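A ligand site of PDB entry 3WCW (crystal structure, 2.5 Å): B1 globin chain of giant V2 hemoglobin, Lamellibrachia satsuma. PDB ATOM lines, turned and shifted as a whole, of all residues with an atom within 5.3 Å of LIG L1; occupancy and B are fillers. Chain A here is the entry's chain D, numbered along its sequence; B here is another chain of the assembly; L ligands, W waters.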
ATOM      1  N   PHE A  37       3.197  -0.663 -34.611  1.00  0.00           N
ATOM      2  CA  PHE A  37       3.166  -1.072 -33.212  1.00  0.00           C
ATOM      3  C   PHE A  37       3.659  -2.500 -32.958  1.00  0.00           C
ATOM      4  O   PHE A  37       4.283  -2.750 -31.924  1.00  0.00           O
ATOM      5  CB  PHE A  37       1.776  -0.843 -32.643  1.00  0.00           C
ATOM      6  CG  PHE A  37       1.531   0.569 -32.244  1.00  0.00           C
ATOM      7  CD1 PHE A  37       1.948   1.034 -30.998  1.00  0.00           C
ATOM      8  CD2 PHE A  37       0.986   1.474 -33.148  1.00  0.00           C
ATOM      9  CE1 PHE A  37       1.825   2.384 -30.659  1.00  0.00           C
ATOM     10  CE2 PHE A  37       0.858   2.824 -32.816  1.00  0.00           C
ATOM     11  CZ  PHE A  37       1.278   3.279 -31.572  1.00  0.00           C
ATOM     12  N   LEU A  40       7.217  -1.999 -32.860  1.00  0.00           N
ATOM     13  CA  LEU A  40       7.665  -1.299 -31.659  1.00  0.00           C
ATOM     14  C   LEU A  40       7.753  -2.299 -30.511  1.00  0.00           C
ATOM     15  O   LEU A  40       8.675  -2.264 -29.699  1.00  0.00           O
ATOM     16  CB  LEU A  40       6.683  -0.195 -31.267  1.00  0.00           C
ATOM     17  CG  LEU A  40       7.122   0.527 -29.992  1.00  0.00           C
ATOM     18  CD1 LEU A  40       8.377   1.323 -30.273  1.00  0.00           C
ATOM     19  CD2 LEU A  40       6.014   1.432 -29.486  1.00  0.00           C
ATOM     20  N   SER A  47       6.816  -2.138 -23.416  1.00  0.00           N
ATOM     21  CA  SER A  47       5.901  -1.024 -23.664  1.00  0.00           C
ATOM     22  C   SER A  47       4.498  -1.505 -24.073  1.00  0.00           C
ATOM     23  O   SER A  47       3.519  -0.763 -23.954  1.00  0.00           O
ATOM     24  CB  SER A  47       6.464  -0.116 -24.766  1.00  0.00           C
ATOM     25  OG  SER A  47       6.544  -0.793 -25.998  1.00  0.00           O
ATOM     26  N   LEU A  50       1.711  -0.836 -21.750  1.00  0.00           N
ATOM     27  CA  LEU A  50       1.227   0.537 -21.741  1.00  0.00           C
ATOM     28  C   LEU A  50      -0.057   0.735 -22.561  1.00  0.00           C
ATOM     29  O   LEU A  50      -0.789   1.693 -22.349  1.00  0.00           O
ATOM     30  CB  LEU A  50       2.311   1.501 -22.253  1.00  0.00           C
ATOM     31  CG  LEU A  50       3.645   1.568 -21.505  1.00  0.00           C
ATOM     32  CD1 LEU A  50       4.573   2.542 -22.204  1.00  0.00           C
ATOM     33  CD2 LEU A  50       3.423   2.012 -20.074  1.00  0.00           C
ATOM     34  N   PHE A  51      -0.316  -0.162 -23.504  1.00  0.00           N
ATOM     35  CA  PHE A  51      -1.488  -0.042 -24.352  1.00  0.00           C
ATOM     36  C   PHE A  51      -2.669  -0.912 -23.931  1.00  0.00           C
ATOM     37  O   PHE A  51      -3.481  -1.320 -24.774  1.00  0.00           O
ATOM     38  CB  PHE A  51      -1.102  -0.325 -25.809  1.00  0.00           C
ATOM     39  CG  PHE A  51       0.032   0.525 -26.293  1.00  0.00           C
ATOM     40  CD1 PHE A  51       1.354   0.074 -26.210  1.00  0.00           C
ATOM     41  CD2 PHE A  51      -0.210   1.821 -26.754  1.00  0.00           C
ATOM     42  CE1 PHE A  51       2.409   0.899 -26.581  1.00  0.00           C
ATOM     43  CE2 PHE A  51       0.846   2.646 -27.125  1.00  0.00           C
ATOM     44  CZ  PHE A  51       2.163   2.182 -27.037  1.00  0.00           C
ATOM     45  N   ASN A  53      -5.403  -0.113 -22.013  1.00  0.00           N
ATOM     46  CA  ASN A  53      -6.730   0.484 -22.097  1.00  0.00           C
ATOM     47  C   ASN A  53      -7.335   0.511 -23.489  1.00  0.00           C
ATOM     48  O   ASN A  53      -8.546   0.688 -23.638  1.00  0.00           O
ATOM     49  CB  ASN A  53      -6.747   1.897 -21.510  1.00  0.00           C
ATOM     50  CG  ASN A  53      -7.151   1.911 -20.047  1.00  0.00           C
ATOM     51  OD1 ASN A  53      -6.423   1.416 -19.185  1.00  0.00           O
ATOM     52  ND2 ASN A  53      -8.331   2.468 -19.768  1.00  0.00           N
ATOM     53  N   VAL A  54      -6.496   0.331 -24.520  1.00  0.00           N
ATOM     54  CA  VAL A  54      -6.986   0.307 -25.885  1.00  0.00           C
ATOM     55  C   VAL A  54      -6.937  -1.121 -26.432  1.00  0.00           C
ATOM     56  O   VAL A  54      -6.822  -1.346 -27.638  1.00  0.00           O
ATOM     57  CB  VAL A  54      -6.199   1.258 -26.802  1.00  0.00           C
ATOM     58  CG1 VAL A  54      -6.514   2.691 -26.419  1.00  0.00           C
ATOM     59  CG2 VAL A  54      -4.698   0.969 -26.719  1.00  0.00           C
ATOM     60  N   HIS A  67      -7.056   3.272 -31.894  1.00  0.00           N
ATOM     61  CA  HIS A  67      -5.881   3.881 -31.281  1.00  0.00           C
ATOM     62  C   HIS A  67      -4.851   4.240 -32.361  1.00  0.00           C
ATOM     63  O   HIS A  67      -4.429   5.397 -32.469  1.00  0.00           O
ATOM     64  CB  HIS A  67      -5.235   2.955 -30.260  1.00  0.00           C
ATOM     65  CG  HIS A  67      -3.929   3.467 -29.733  1.00  0.00           C
ATOM     66  ND1 HIS A  67      -3.829   4.604 -28.964  1.00  0.00           N
ATOM     67  CD2 HIS A  67      -2.665   3.024 -29.936  1.00  0.00           C
ATOM     68  CE1 HIS A  67      -2.555   4.848 -28.710  1.00  0.00           C
ATOM     69  NE2 HIS A  67      -1.827   3.903 -29.291  1.00  0.00           N
ATOM     70  N   ARG A  70      -5.764   6.937 -34.581  1.00  0.00           N
ATOM     71  CA  ARG A  70      -5.582   8.165 -33.827  1.00  0.00           C
ATOM     72  C   ARG A  70      -4.112   8.622 -33.816  1.00  0.00           C
ATOM     73  O   ARG A  70      -3.822   9.825 -33.868  1.00  0.00           O
ATOM     74  CB  ARG A  70      -6.087   7.920 -32.415  1.00  0.00           C
ATOM     75  CG  ARG A  70      -6.655   9.102 -31.688  1.00  0.00           C
ATOM     76  CD  ARG A  70      -7.276   8.637 -30.346  1.00  0.00           C
ATOM     77  NE  ARG A  70      -8.436   7.784 -30.573  1.00  0.00           N
ATOM     78  CZ  ARG A  70      -8.678   6.662 -29.904  1.00  0.00           C
ATOM     79  NH1 ARG A  70      -7.845   6.235 -28.961  1.00  0.00           N
ATOM     80  NH2 ARG A  70      -9.780   5.959 -30.184  1.00  0.00           N
ATOM     81  N   VAL A  71      -3.188   7.665 -33.746  1.00  0.00           N
ATOM     82  CA  VAL A  71      -1.757   7.980 -33.706  1.00  0.00           C
ATOM     83  C   VAL A  71      -1.241   8.435 -35.076  1.00  0.00           C
ATOM     84  O   VAL A  71      -0.514   9.437 -35.196  1.00  0.00           O
ATOM     85  CB  VAL A  71      -0.935   6.731 -33.242  1.00  0.00           C
ATOM     86  CG1 VAL A  71       0.560   6.989 -33.381  1.00  0.00           C
ATOM     87  CG2 VAL A  71      -1.294   6.391 -31.782  1.00  0.00           C
ATOM     88  N   GLY A  74      -2.217  11.866 -35.616  1.00  0.00           N
ATOM     89  CA  GLY A  74      -1.396  12.863 -34.949  1.00  0.00           C
ATOM     90  C   GLY A  74      -0.140  13.100 -35.767  1.00  0.00           C
ATOM     91  O   GLY A  74       0.278  14.236 -36.002  1.00  0.00           O
ATOM     92  N   LEU A  75       0.480  12.001 -36.203  1.00  0.00           N
ATOM     93  CA  LEU A  75       1.697  12.076 -37.002  1.00  0.00           C
ATOM     94  C   LEU A  75       1.368  12.914 -38.241  1.00  0.00           C
ATOM     95  O   LEU A  75       2.158  13.754 -38.658  1.00  0.00           O
ATOM     96  CB  LEU A  75       2.113  10.657 -37.416  1.00  0.00           C
ATOM     97  CG  LEU A  75       3.453  10.454 -38.098  1.00  0.00           C
ATOM     98  CD1 LEU A  75       4.577  10.891 -37.172  1.00  0.00           C
ATOM     99  CD2 LEU A  75       3.609   8.988 -38.435  1.00  0.00           C
ATOM    100  N   LEU A  95       0.677  17.140 -27.599  1.00  0.00           N
ATOM    101  CA  LEU A  95       0.982  15.725 -27.763  1.00  0.00           C
ATOM    102  C   LEU A  95       1.865  15.231 -26.618  1.00  0.00           C
ATOM    103  O   LEU A  95       1.695  14.116 -26.116  1.00  0.00           O
ATOM    104  CB  LEU A  95       1.699  15.483 -29.103  1.00  0.00           C
ATOM    105  CG  LEU A  95       0.776  15.316 -30.306  1.00  0.00           C
ATOM    106  CD1 LEU A  95       1.572  15.179 -31.601  1.00  0.00           C
ATOM    107  CD2 LEU A  95      -0.078  14.094 -30.069  1.00  0.00           C
ATOM    108  N   GLN A  98      -0.077  14.651 -23.535  1.00  0.00           N
ATOM    109  CA  GLN A  98      -0.850  13.425 -23.647  1.00  0.00           C
ATOM    110  C   GLN A  98      -0.005  12.174 -23.411  1.00  0.00           C
ATOM    111  O   GLN A  98      -0.544  11.084 -23.176  1.00  0.00           O
ATOM    112  CB  GLN A  98      -1.523  13.333 -25.019  1.00  0.00           C
ATOM    113  CG  GLN A  98      -2.570  14.424 -25.251  1.00  0.00           C
ATOM    114  CD  GLN A  98      -3.172  14.369 -26.648  1.00  0.00           C
ATOM    115  OE1 GLN A  98      -2.452  14.378 -27.636  1.00  0.00           O
ATOM    116  NE2 GLN A  98      -4.500  14.322 -26.722  1.00  0.00           N
ATOM    117  N   HIS A  99       1.318  12.317 -23.476  1.00  0.00           N
ATOM    118  CA  HIS A  99       2.157  11.150 -23.257  1.00  0.00           C
ATOM    119  C   HIS A  99       2.776  11.107 -21.872  1.00  0.00           C
ATOM    120  O   HIS A  99       2.801  10.053 -21.238  1.00  0.00           O
ATOM    121  CB  HIS A  99       3.247  11.054 -24.339  1.00  0.00           C
ATOM    122  CG  HIS A  99       2.736  10.512 -25.635  1.00  0.00           C
ATOM    123  ND1 HIS A  99       2.070  11.286 -26.567  1.00  0.00           N
ATOM    124  CD2 HIS A  99       2.724   9.249 -26.124  1.00  0.00           C
ATOM    125  CE1 HIS A  99       1.661  10.525 -27.559  1.00  0.00           C
ATOM    126  NE2 HIS A  99       2.042   9.286 -27.325  1.00  0.00           N
ATOM    127  N   ARG A 102       0.941   9.373 -19.246  1.00  0.00           N
ATOM    128  CA  ARG A 102       0.979   7.920 -19.246  1.00  0.00           C
ATOM    129  C   ARG A 102       2.214   7.428 -18.495  1.00  0.00           C
ATOM    130  O   ARG A 102       3.314   7.379 -19.051  1.00  0.00           O
ATOM    131  CB  ARG A 102       1.005   7.383 -20.684  1.00  0.00           C
ATOM    132  CG  ARG A 102      -0.031   8.009 -21.626  1.00  0.00           C
ATOM    133  CD  ARG A 102      -1.468   7.742 -21.201  1.00  0.00           C
ATOM    134  NE  ARG A 102      -1.737   6.313 -21.043  1.00  0.00           N
ATOM    135  CZ  ARG A 102      -2.947   5.764 -20.984  1.00  0.00           C
ATOM    136  NH1 ARG A 102      -4.037   6.532 -21.070  1.00  0.00           N
ATOM    137  NH2 ARG A 102      -3.079   4.455 -20.854  1.00  0.00           N
ATOM    138  N   LEU A 105       5.960   5.516 -19.630  1.00  0.00           N
ATOM    139  CA  LEU A 105       6.488   5.947 -20.921  1.00  0.00           C
ATOM    140  C   LEU A 105       7.900   6.481 -20.822  1.00  0.00           C
ATOM    141  O   LEU A 105       8.139   7.568 -20.269  1.00  0.00           O
ATOM    142  CB  LEU A 105       5.601   7.029 -21.518  1.00  0.00           C
ATOM    143  CG  LEU A 105       5.262   6.800 -22.982  1.00  0.00           C
ATOM    144  CD1 LEU A 105       4.305   5.611 -23.100  1.00  0.00           C
ATOM    145  CD2 LEU A 105       4.629   8.036 -23.567  1.00  0.00           C
ATOM    146  N   TYR A 109      11.606   4.881 -25.508  1.00  0.00           N
ATOM    147  CA  TYR A 109      10.591   4.190 -26.286  1.00  0.00           C
ATOM    148  C   TYR A 109      10.301   4.990 -27.545  1.00  0.00           C
ATOM    149  O   TYR A 109       9.967   4.427 -28.595  1.00  0.00           O
ATOM    150  CB  TYR A 109       9.295   4.027 -25.485  1.00  0.00           C
ATOM    151  CG  TYR A 109       9.384   3.077 -24.308  1.00  0.00           C
ATOM    152  CD1 TYR A 109      10.353   2.063 -24.260  1.00  0.00           C
ATOM    153  CD2 TYR A 109       8.476   3.171 -23.259  1.00  0.00           C
ATOM    154  CE1 TYR A 109      10.397   1.160 -23.178  1.00  0.00           C
ATOM    155  CE2 TYR A 109       8.508   2.286 -22.183  1.00  0.00           C
ATOM    156  CZ  TYR A 109       9.463   1.280 -22.151  1.00  0.00           C
ATOM    157  OH  TYR A 109       9.472   0.389 -21.095  1.00  0.00           O
ATOM    158  N   PHE A 110      10.421   6.314 -27.442  1.00  0.00           N
ATOM    159  CA  PHE A 110      10.191   7.185 -28.592  1.00  0.00           C
ATOM    160  C   PHE A 110      11.304   7.050 -29.625  1.00  0.00           C
ATOM    161  O   PHE A 110      11.088   7.306 -30.802  1.00  0.00           O
ATOM    162  CB  PHE A 110      10.068   8.643 -28.156  1.00  0.00           C
ATOM    163  CG  PHE A 110       8.645   9.106 -28.044  1.00  0.00           C
ATOM    164  CD1 PHE A 110       7.840   8.654 -27.003  1.00  0.00           C
ATOM    165  CD2 PHE A 110       8.086   9.929 -29.014  1.00  0.00           C
ATOM    166  CE1 PHE A 110       6.487   9.018 -26.938  1.00  0.00           C
ATOM    167  CE2 PHE A 110       6.744  10.287 -28.955  1.00  0.00           C
ATOM    168  CZ  PHE A 110       5.942   9.825 -27.915  1.00  0.00           C
ATOM    169  N   MET A 113      10.469   4.009 -31.651  1.00  0.00           N
ATOM    170  CA  MET A 113       9.416   4.317 -32.630  1.00  0.00           C
ATOM    171  C   MET A 113      10.094   4.966 -33.838  1.00  0.00           C
ATOM    172  O   MET A 113       9.780   4.652 -34.998  1.00  0.00           O
ATOM    173  CB  MET A 113       8.366   5.252 -32.022  1.00  0.00           C
ATOM    174  CG  MET A 113       7.212   5.681 -32.950  1.00  0.00           C
ATOM    175  SD  MET A 113       6.019   4.383 -33.477  1.00  0.00           S
ATOM    176  CE  MET A 113       4.774   4.567 -32.293  1.00  0.00           C
ATOM    177  N   LEU A 117       9.708   3.705 -37.630  1.00  0.00           N
ATOM    178  CA  LEU A 117       9.193   4.452 -38.763  1.00  0.00           C
ATOM    179  C   LEU A 117      10.221   4.446 -39.886  1.00  0.00           C
ATOM    180  O   LEU A 117       9.883   4.176 -41.036  1.00  0.00           O
ATOM    181  CB  LEU A 117       8.833   5.877 -38.339  1.00  0.00           C
ATOM    182  CG  LEU A 117       7.628   5.961 -37.396  1.00  0.00           C
ATOM    183  CD1 LEU A 117       7.383   7.389 -36.951  1.00  0.00           C
ATOM    184  CD2 LEU A 117       6.392   5.404 -38.107  1.00  0.00           C
ATOM    185  N   LYS A 141       9.993  14.223 -32.902  1.00  0.00           N
ATOM    186  CA  LYS A 141      10.167  13.209 -31.879  1.00  0.00           C
ATOM    187  C   LYS A 141      10.663  13.787 -30.565  1.00  0.00           C
ATOM    188  O   LYS A 141      10.117  13.470 -29.514  1.00  0.00           O
ATOM    189  CB  LYS A 141      11.113  12.116 -32.393  1.00  0.00           C
ATOM    190  CG  LYS A 141      11.158  10.846 -31.535  1.00  0.00           C
ATOM    191  CD  LYS A 141      12.442  10.775 -30.716  1.00  0.00           C
ATOM    192  CE  LYS A 141      13.664  10.617 -31.602  1.00  0.00           C
ATOM    193  NZ  LYS A 141      14.953  10.754 -30.845  1.00  0.00           N
ATOM    194  N   ILE A 144       7.848  15.794 -28.868  1.00  0.00           N
ATOM    195  CA  ILE A 144       6.730  15.019 -28.355  1.00  0.00           C
ATOM    196  C   ILE A 144       7.137  14.237 -27.101  1.00  0.00           C
ATOM    197  O   ILE A 144       6.333  14.020 -26.205  1.00  0.00           O
ATOM    198  CB  ILE A 144       6.177  14.029 -29.409  1.00  0.00           C
ATOM    199  CG1 ILE A 144       5.551  14.817 -30.571  1.00  0.00           C
ATOM    200  CG2 ILE A 144       5.140  13.101 -28.788  1.00  0.00           C
ATOM    201  CD1 ILE A 144       4.956  13.923 -31.668  1.00  0.00           C
ATOM    202  N   HIS B  89     -14.159   7.654 -27.474  1.00  0.00           N
ATOM    203  CA  HIS B  89     -12.928   8.296 -27.020  1.00  0.00           C
ATOM    204  C   HIS B  89     -13.148   9.812 -27.065  1.00  0.00           C
ATOM    205  O   HIS B  89     -12.772  10.537 -26.143  1.00  0.00           O
ATOM    206  CB  HIS B  89     -11.765   7.902 -27.939  1.00  0.00           C
ATOM    207  CG  HIS B  89     -10.435   8.418 -27.487  1.00  0.00           C
ATOM    208  ND1 HIS B  89      -9.650   7.756 -26.560  1.00  0.00           N
ATOM    209  CD2 HIS B  89      -9.738   9.517 -27.837  1.00  0.00           C
ATOM    210  CE1 HIS B  89      -8.540   8.437 -26.354  1.00  0.00           C
ATOM    211  NE2 HIS B  89      -8.564   9.516 -27.122  1.00  0.00           N
ATOM    212  N   GLN B  93     -13.669  12.905 -24.056  1.00  0.00           N
ATOM    213  CA  GLN B  93     -12.975  14.173 -23.981  1.00  0.00           C
ATOM    214  C   GLN B  93     -13.946  15.347 -23.961  1.00  0.00           C
ATOM    215  O   GLN B  93     -13.636  16.393 -23.401  1.00  0.00           O
ATOM    216  CB  GLN B  93     -11.999  14.334 -25.160  1.00  0.00           C
ATOM    217  CG  GLN B  93     -10.850  13.366 -25.101  1.00  0.00           C
ATOM    218  CD  GLN B  93     -10.081  13.274 -26.408  1.00  0.00           C
ATOM    219  OE1 GLN B  93     -10.665  13.022 -27.462  1.00  0.00           O
ATOM    220  NE2 GLN B  93      -8.766  13.464 -26.329  1.00  0.00           N
HETATM  221  C1  LIG L   1      -1.721   7.952 -27.227  1.00  0.00           C
HETATM  222  C2  LIG L   1       0.443   9.873 -31.014  1.00  0.00           C
HETATM  223  C3  LIG L   1       4.516   7.485 -29.983  1.00  0.00           C
HETATM  224  C4  LIG L   1       2.337   5.605 -26.119  1.00  0.00           C
HETATM  225  C5  LIG L   1      -1.503   8.701 -28.365  1.00  0.00           C
HETATM  226  C6  LIG L   1      -2.486   9.500 -28.965  1.00  0.00           C
HETATM  227  C7  LIG L   1      -1.889  10.069 -30.041  1.00  0.00           C
HETATM  228  C8  LIG L   1      -0.495   9.592 -30.108  1.00  0.00           C
HETATM  229  C9  LIG L   1      -2.529  11.038 -31.046  1.00  0.00           C
HETATM  230  C10 LIG L   1      -3.921   9.696 -28.519  1.00  0.00           C
HETATM  231  C11 LIG L   1      -4.157  10.948 -27.750  1.00  0.00           C
HETATM  232  C12 LIG L   1      -5.607  11.117 -27.304  1.00  0.00           C
HETATM  233  O1  LIG L   1      -5.950  10.699 -26.181  1.00  0.00           O
HETATM  234  O2  LIG L   1      -6.378  11.620 -28.056  1.00  0.00           O
HETATM  235  C13 LIG L   1       1.781   9.401 -31.106  1.00  0.00           C
HETATM  236  C14 LIG L   1       2.707   9.767 -32.168  1.00  0.00           C
HETATM  237  C15 LIG L   1       3.916   9.036 -31.851  1.00  0.00           C
HETATM  238  C16 LIG L   1       3.611   8.327 -30.649  1.00  0.00           C
HETATM  239  C17 LIG L   1       2.448  10.682 -33.316  1.00  0.00           C
HETATM  240  C18 LIG L   1       5.117   9.096 -32.663  1.00  0.00           C
HETATM  241  C19 LIG L   1       6.219   9.719 -32.315  1.00  0.00           C
HETATM  242  C20 LIG L   1       4.259   6.775 -28.824  1.00  0.00           C
HETATM  243  C21 LIG L   1       5.277   5.909 -28.191  1.00  0.00           C
HETATM  244  C22 LIG L   1       4.681   5.334 -27.044  1.00  0.00           C
HETATM  245  C23 LIG L   1       3.266   5.918 -27.058  1.00  0.00           C
HETATM  246  C24 LIG L   1       6.696   5.695 -28.709  1.00  0.00           C
HETATM  247  C25 LIG L   1       5.232   4.475 -26.161  1.00  0.00           C
HETATM  248  C26 LIG L   1       5.414   3.212 -26.011  1.00  0.00           C
HETATM  249  C27 LIG L   1       1.025   6.080 -26.080  1.00  0.00           C
HETATM  250  C28 LIG L   1       0.023   5.689 -25.014  1.00  0.00           C
HETATM  251  C29 LIG L   1      -1.117   6.360 -25.357  1.00  0.00           C
HETATM  252  C30 LIG L   1      -0.815   7.144 -26.577  1.00  0.00           C
HETATM  253  C31 LIG L   1       0.308   4.729 -23.854  1.00  0.00           C
HETATM  254  C32 LIG L   1      -2.447   6.320 -24.631  1.00  0.00           C
HETATM  255  C33 LIG L   1      -3.313   5.186 -25.124  1.00  0.00           C
HETATM  256  C34 LIG L   1      -4.624   5.113 -24.443  1.00  0.00           C
HETATM  257  O3  LIG L   1      -5.514   6.001 -24.670  1.00  0.00           O
HETATM  258  O4  LIG L   1      -4.839   4.155 -23.641  1.00  0.00           O
HETATM  259  N1  LIG L   1      -0.274   8.748 -29.051  1.00  0.00           N
HETATM  260  N2  LIG L   1       2.287   8.558 -30.207  1.00  0.00           N
HETATM  261  N3  LIG L   1       3.070   6.748 -28.106  1.00  0.00           N
HETATM  262  N4  LIG L   1       0.482   6.941 -26.969  1.00  0.00           N
HETATM  263 FE1  LIG L   1       1.398   7.758 -28.573  1.00  0.00          FE
HETATM  264  O1  LG2 L   2       0.843   6.420 -29.637  1.00  0.00           O
HETATM  265  O2  LG2 L   2       0.935   5.231 -29.354  1.00  0.00           O
HETATM  266  C1  LG3 L   3     -11.422  19.417 -28.077  1.00  0.00           C
HETATM  267  C2  LG3 L   3     -13.014  17.112 -31.915  1.00  0.00           C
HETATM  268  C3  LG3 L   3     -17.204  19.451 -31.637  1.00  0.00           C
HETATM  269  C4  LG3 L   3     -15.597  21.733 -27.735  1.00  0.00           C
HETATM  270  C5  LG3 L   3     -11.471  18.580 -29.161  1.00  0.00           C
HETATM  271  C6  LG3 L   3     -10.401  17.768 -29.557  1.00  0.00           C
HETATM  272  C7  LG3 L   3     -10.838  17.102 -30.649  1.00  0.00           C
HETATM  273  C8  LG3 L   3     -12.211  17.514 -30.921  1.00  0.00           C
HETATM  274  C9  LG3 L   3     -10.060  16.082 -31.480  1.00  0.00           C
HETATM  275  C10 LG3 L   3      -9.039  17.664 -28.904  1.00  0.00           C
HETATM  276  C11 LG3 L   3      -8.946  16.494 -27.957  1.00  0.00           C
HETATM  277  C12 LG3 L   3      -7.586  16.376 -27.277  1.00  0.00           C
HETATM  278  O1  LG3 L   3      -7.505  16.524 -26.033  1.00  0.00           O
HETATM  279  O2  LG3 L   3      -6.628  16.168 -27.964  1.00  0.00           O
HETATM  280  C13 LG3 L   3     -14.323  17.525 -32.205  1.00  0.00           C
HETATM  281  C14 LG3 L   3     -15.099  17.029 -33.324  1.00  0.00           C
HETATM  282  C15 LG3 L   3     -16.350  17.739 -33.230  1.00  0.00           C
HETATM  283  C16 LG3 L   3     -16.209  18.578 -32.086  1.00  0.00           C
HETATM  284  C17 LG3 L   3     -14.689  16.014 -34.337  1.00  0.00           C
HETATM  285  C18 LG3 L   3     -17.444  17.566 -34.168  1.00  0.00           C
HETATM  286  C19 LG3 L   3     -18.240  16.528 -34.226  1.00  0.00           C
HETATM  287  C20 LG3 L   3     -17.117  20.279 -30.541  1.00  0.00           C
HETATM  288  C21 LG3 L   3     -18.215  21.176 -30.136  1.00  0.00           C
HETATM  289  C22 LG3 L   3     -17.785  21.855 -28.993  1.00  0.00           C
HETATM  290  C23 LG3 L   3     -16.389  21.317 -28.757  1.00  0.00           C
HETATM  291  C24 LG3 L   3     -19.568  21.320 -30.846  1.00  0.00           C
HETATM  292  C25 LG3 L   3     -18.467  22.791 -28.274  1.00  0.00           C
HETATM  293  C26 LG3 L   3     -18.694  24.059 -28.300  1.00  0.00           C
HETATM  294  C27 LG3 L   3     -14.312  21.295 -27.475  1.00  0.00           C
HETATM  295  C28 LG3 L   3     -13.472  21.809 -26.326  1.00  0.00           C
HETATM  296  C29 LG3 L   3     -12.276  21.127 -26.448  1.00  0.00           C
HETATM  297  C30 LG3 L   3     -12.409  20.240 -27.627  1.00  0.00           C
HETATM  298  C31 LG3 L   3     -13.934  22.850 -25.319  1.00  0.00           C
HETATM  299  C32 LG3 L   3     -11.044  21.233 -25.568  1.00  0.00           C
HETATM  300  C33 LG3 L   3     -10.069  22.273 -26.029  1.00  0.00           C
HETATM  301  C34 LG3 L   3      -8.862  22.344 -25.188  1.00  0.00           C
HETATM  302  O3  LG3 L   3      -8.752  23.219 -24.291  1.00  0.00           O
HETATM  303  O4  LG3 L   3      -7.954  21.525 -25.397  1.00  0.00           O
HETATM  304  N1  LG3 L   3     -12.592  18.440 -29.989  1.00  0.00           N
HETATM  305  N2  LG3 L   3     -14.951  18.433 -31.458  1.00  0.00           N
HETATM  306  N3  LG3 L   3     -16.046  20.409 -29.679  1.00  0.00           N
HETATM  307  N4  LG3 L   3     -13.641  20.378 -28.200  1.00  0.00           N
HETATM  308 FE1  LG3 L   3     -14.317  19.413 -29.810  1.00  0.00          FE
HETATM  309  O   HOH W   1      -5.961  12.766 -30.784  1.00  0.00           O
HETATM  310  O   HOH W   2      -9.206  12.702 -29.805  1.00  0.00           O
HETATM  311  O   HOH W   3      -5.411   6.482 -27.543  1.00  0.00           O
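NE2 of Gln 98 is in hydrogen-bond range of O2 of LG3 L3, at 3.1 Å. O1 of LIG L1 sits at hydrogen-bond distance from NE2 of His 89 of chain B, at 3.0 Å. NE2 of His 67 lies within hydrogen-bond range of O2 of LG2 L2, 3.1 Å away. An iron atom (FE1) of LIG L1 is bound by a ring nitrogen (NE2) of His 99 (2.1 Å). An oxygen (O1) of LG3 L3 sits close to the side-chain amide nitrogen (NE2) of Gln 93 of chain B (3.3 Å). NE2 of Gln 93 of chain B lies within hydrogen-bond range of O2 of LIG L1 (3.5 Å). NH2 of Arg 102 is in salt-bridge range of O4 of LIG L1 (3.3 Å).
FE1 of LIG L1 is bound by O1 of LG2 L2 (1.8 Å).
A ring nitrogen (ND1) of His 89 of chain B is in hydrogen-bond range of the guanidinium group (NH1) of Arg 70 (3.4 Å). The backbone carbonyl oxygen (O) of Leu 95 sits at hydrogen-bond distance from a ring nitrogen (ND1) of His 99 (2.9 Å).
Leu 40 touches LIG L1. Ser 47 touches LIG L1 (CB to C26, 3.7 Å). Leu 50 touches LIG L1 (O to C31, 3.6 Å). CE2 of Phe 51 touches C4 of LIG L1 (3.5 Å). Asn 53 touches LIG L1 (CB to O4, 3.6 Å). Val 54 touches LIG L1. His 67 touches LIG L1 (CE1 to C1, 3.5 Å). Arg 70 touches LIG L1. Val 71 touches LIG L1 (CG1 to C13, 3.5 Å). Leu 75 touches LIG L1 (N to C17, 3.7 Å). Gln 98 touches LIG L1. Leu 105 touches LIG L1 (CD1 to C25, 3.4 Å). O of Tyr 109 touches C24 of LIG L1, at 3.5 Å. CZ of Phe 110 touches C3 of LIG L1, 3.4 Å away. Met 113 touches LIG L1. Hydrophobic or aromatic side chains within 4 Å of LIG L1: Leu 40, Leu 50, Phe 51, Val 54, His 67, Val 71, His 99, Leu 105, Phe 110, Met 113 and His 89 of chain B. Of the 25 residues printed, 19 come within 4 Å of LIG L1. The nearest printed residue that does not touch LIG L1 is Leu 95 (4.04 Å).
Water W3 lies within hydrogen-bond range of the guanidinium group (NH1) of Arg 70, a ring nitrogen (ND1) of His 67 and an oxygen (O3) of LIG L1. Water W2 lies within hydrogen-bond range of the side-chain amide oxygen (OE1) of Gln 93 of chain B (2.8 Å) and an oxygen (O2) of LIG L1 (3.5 Å).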
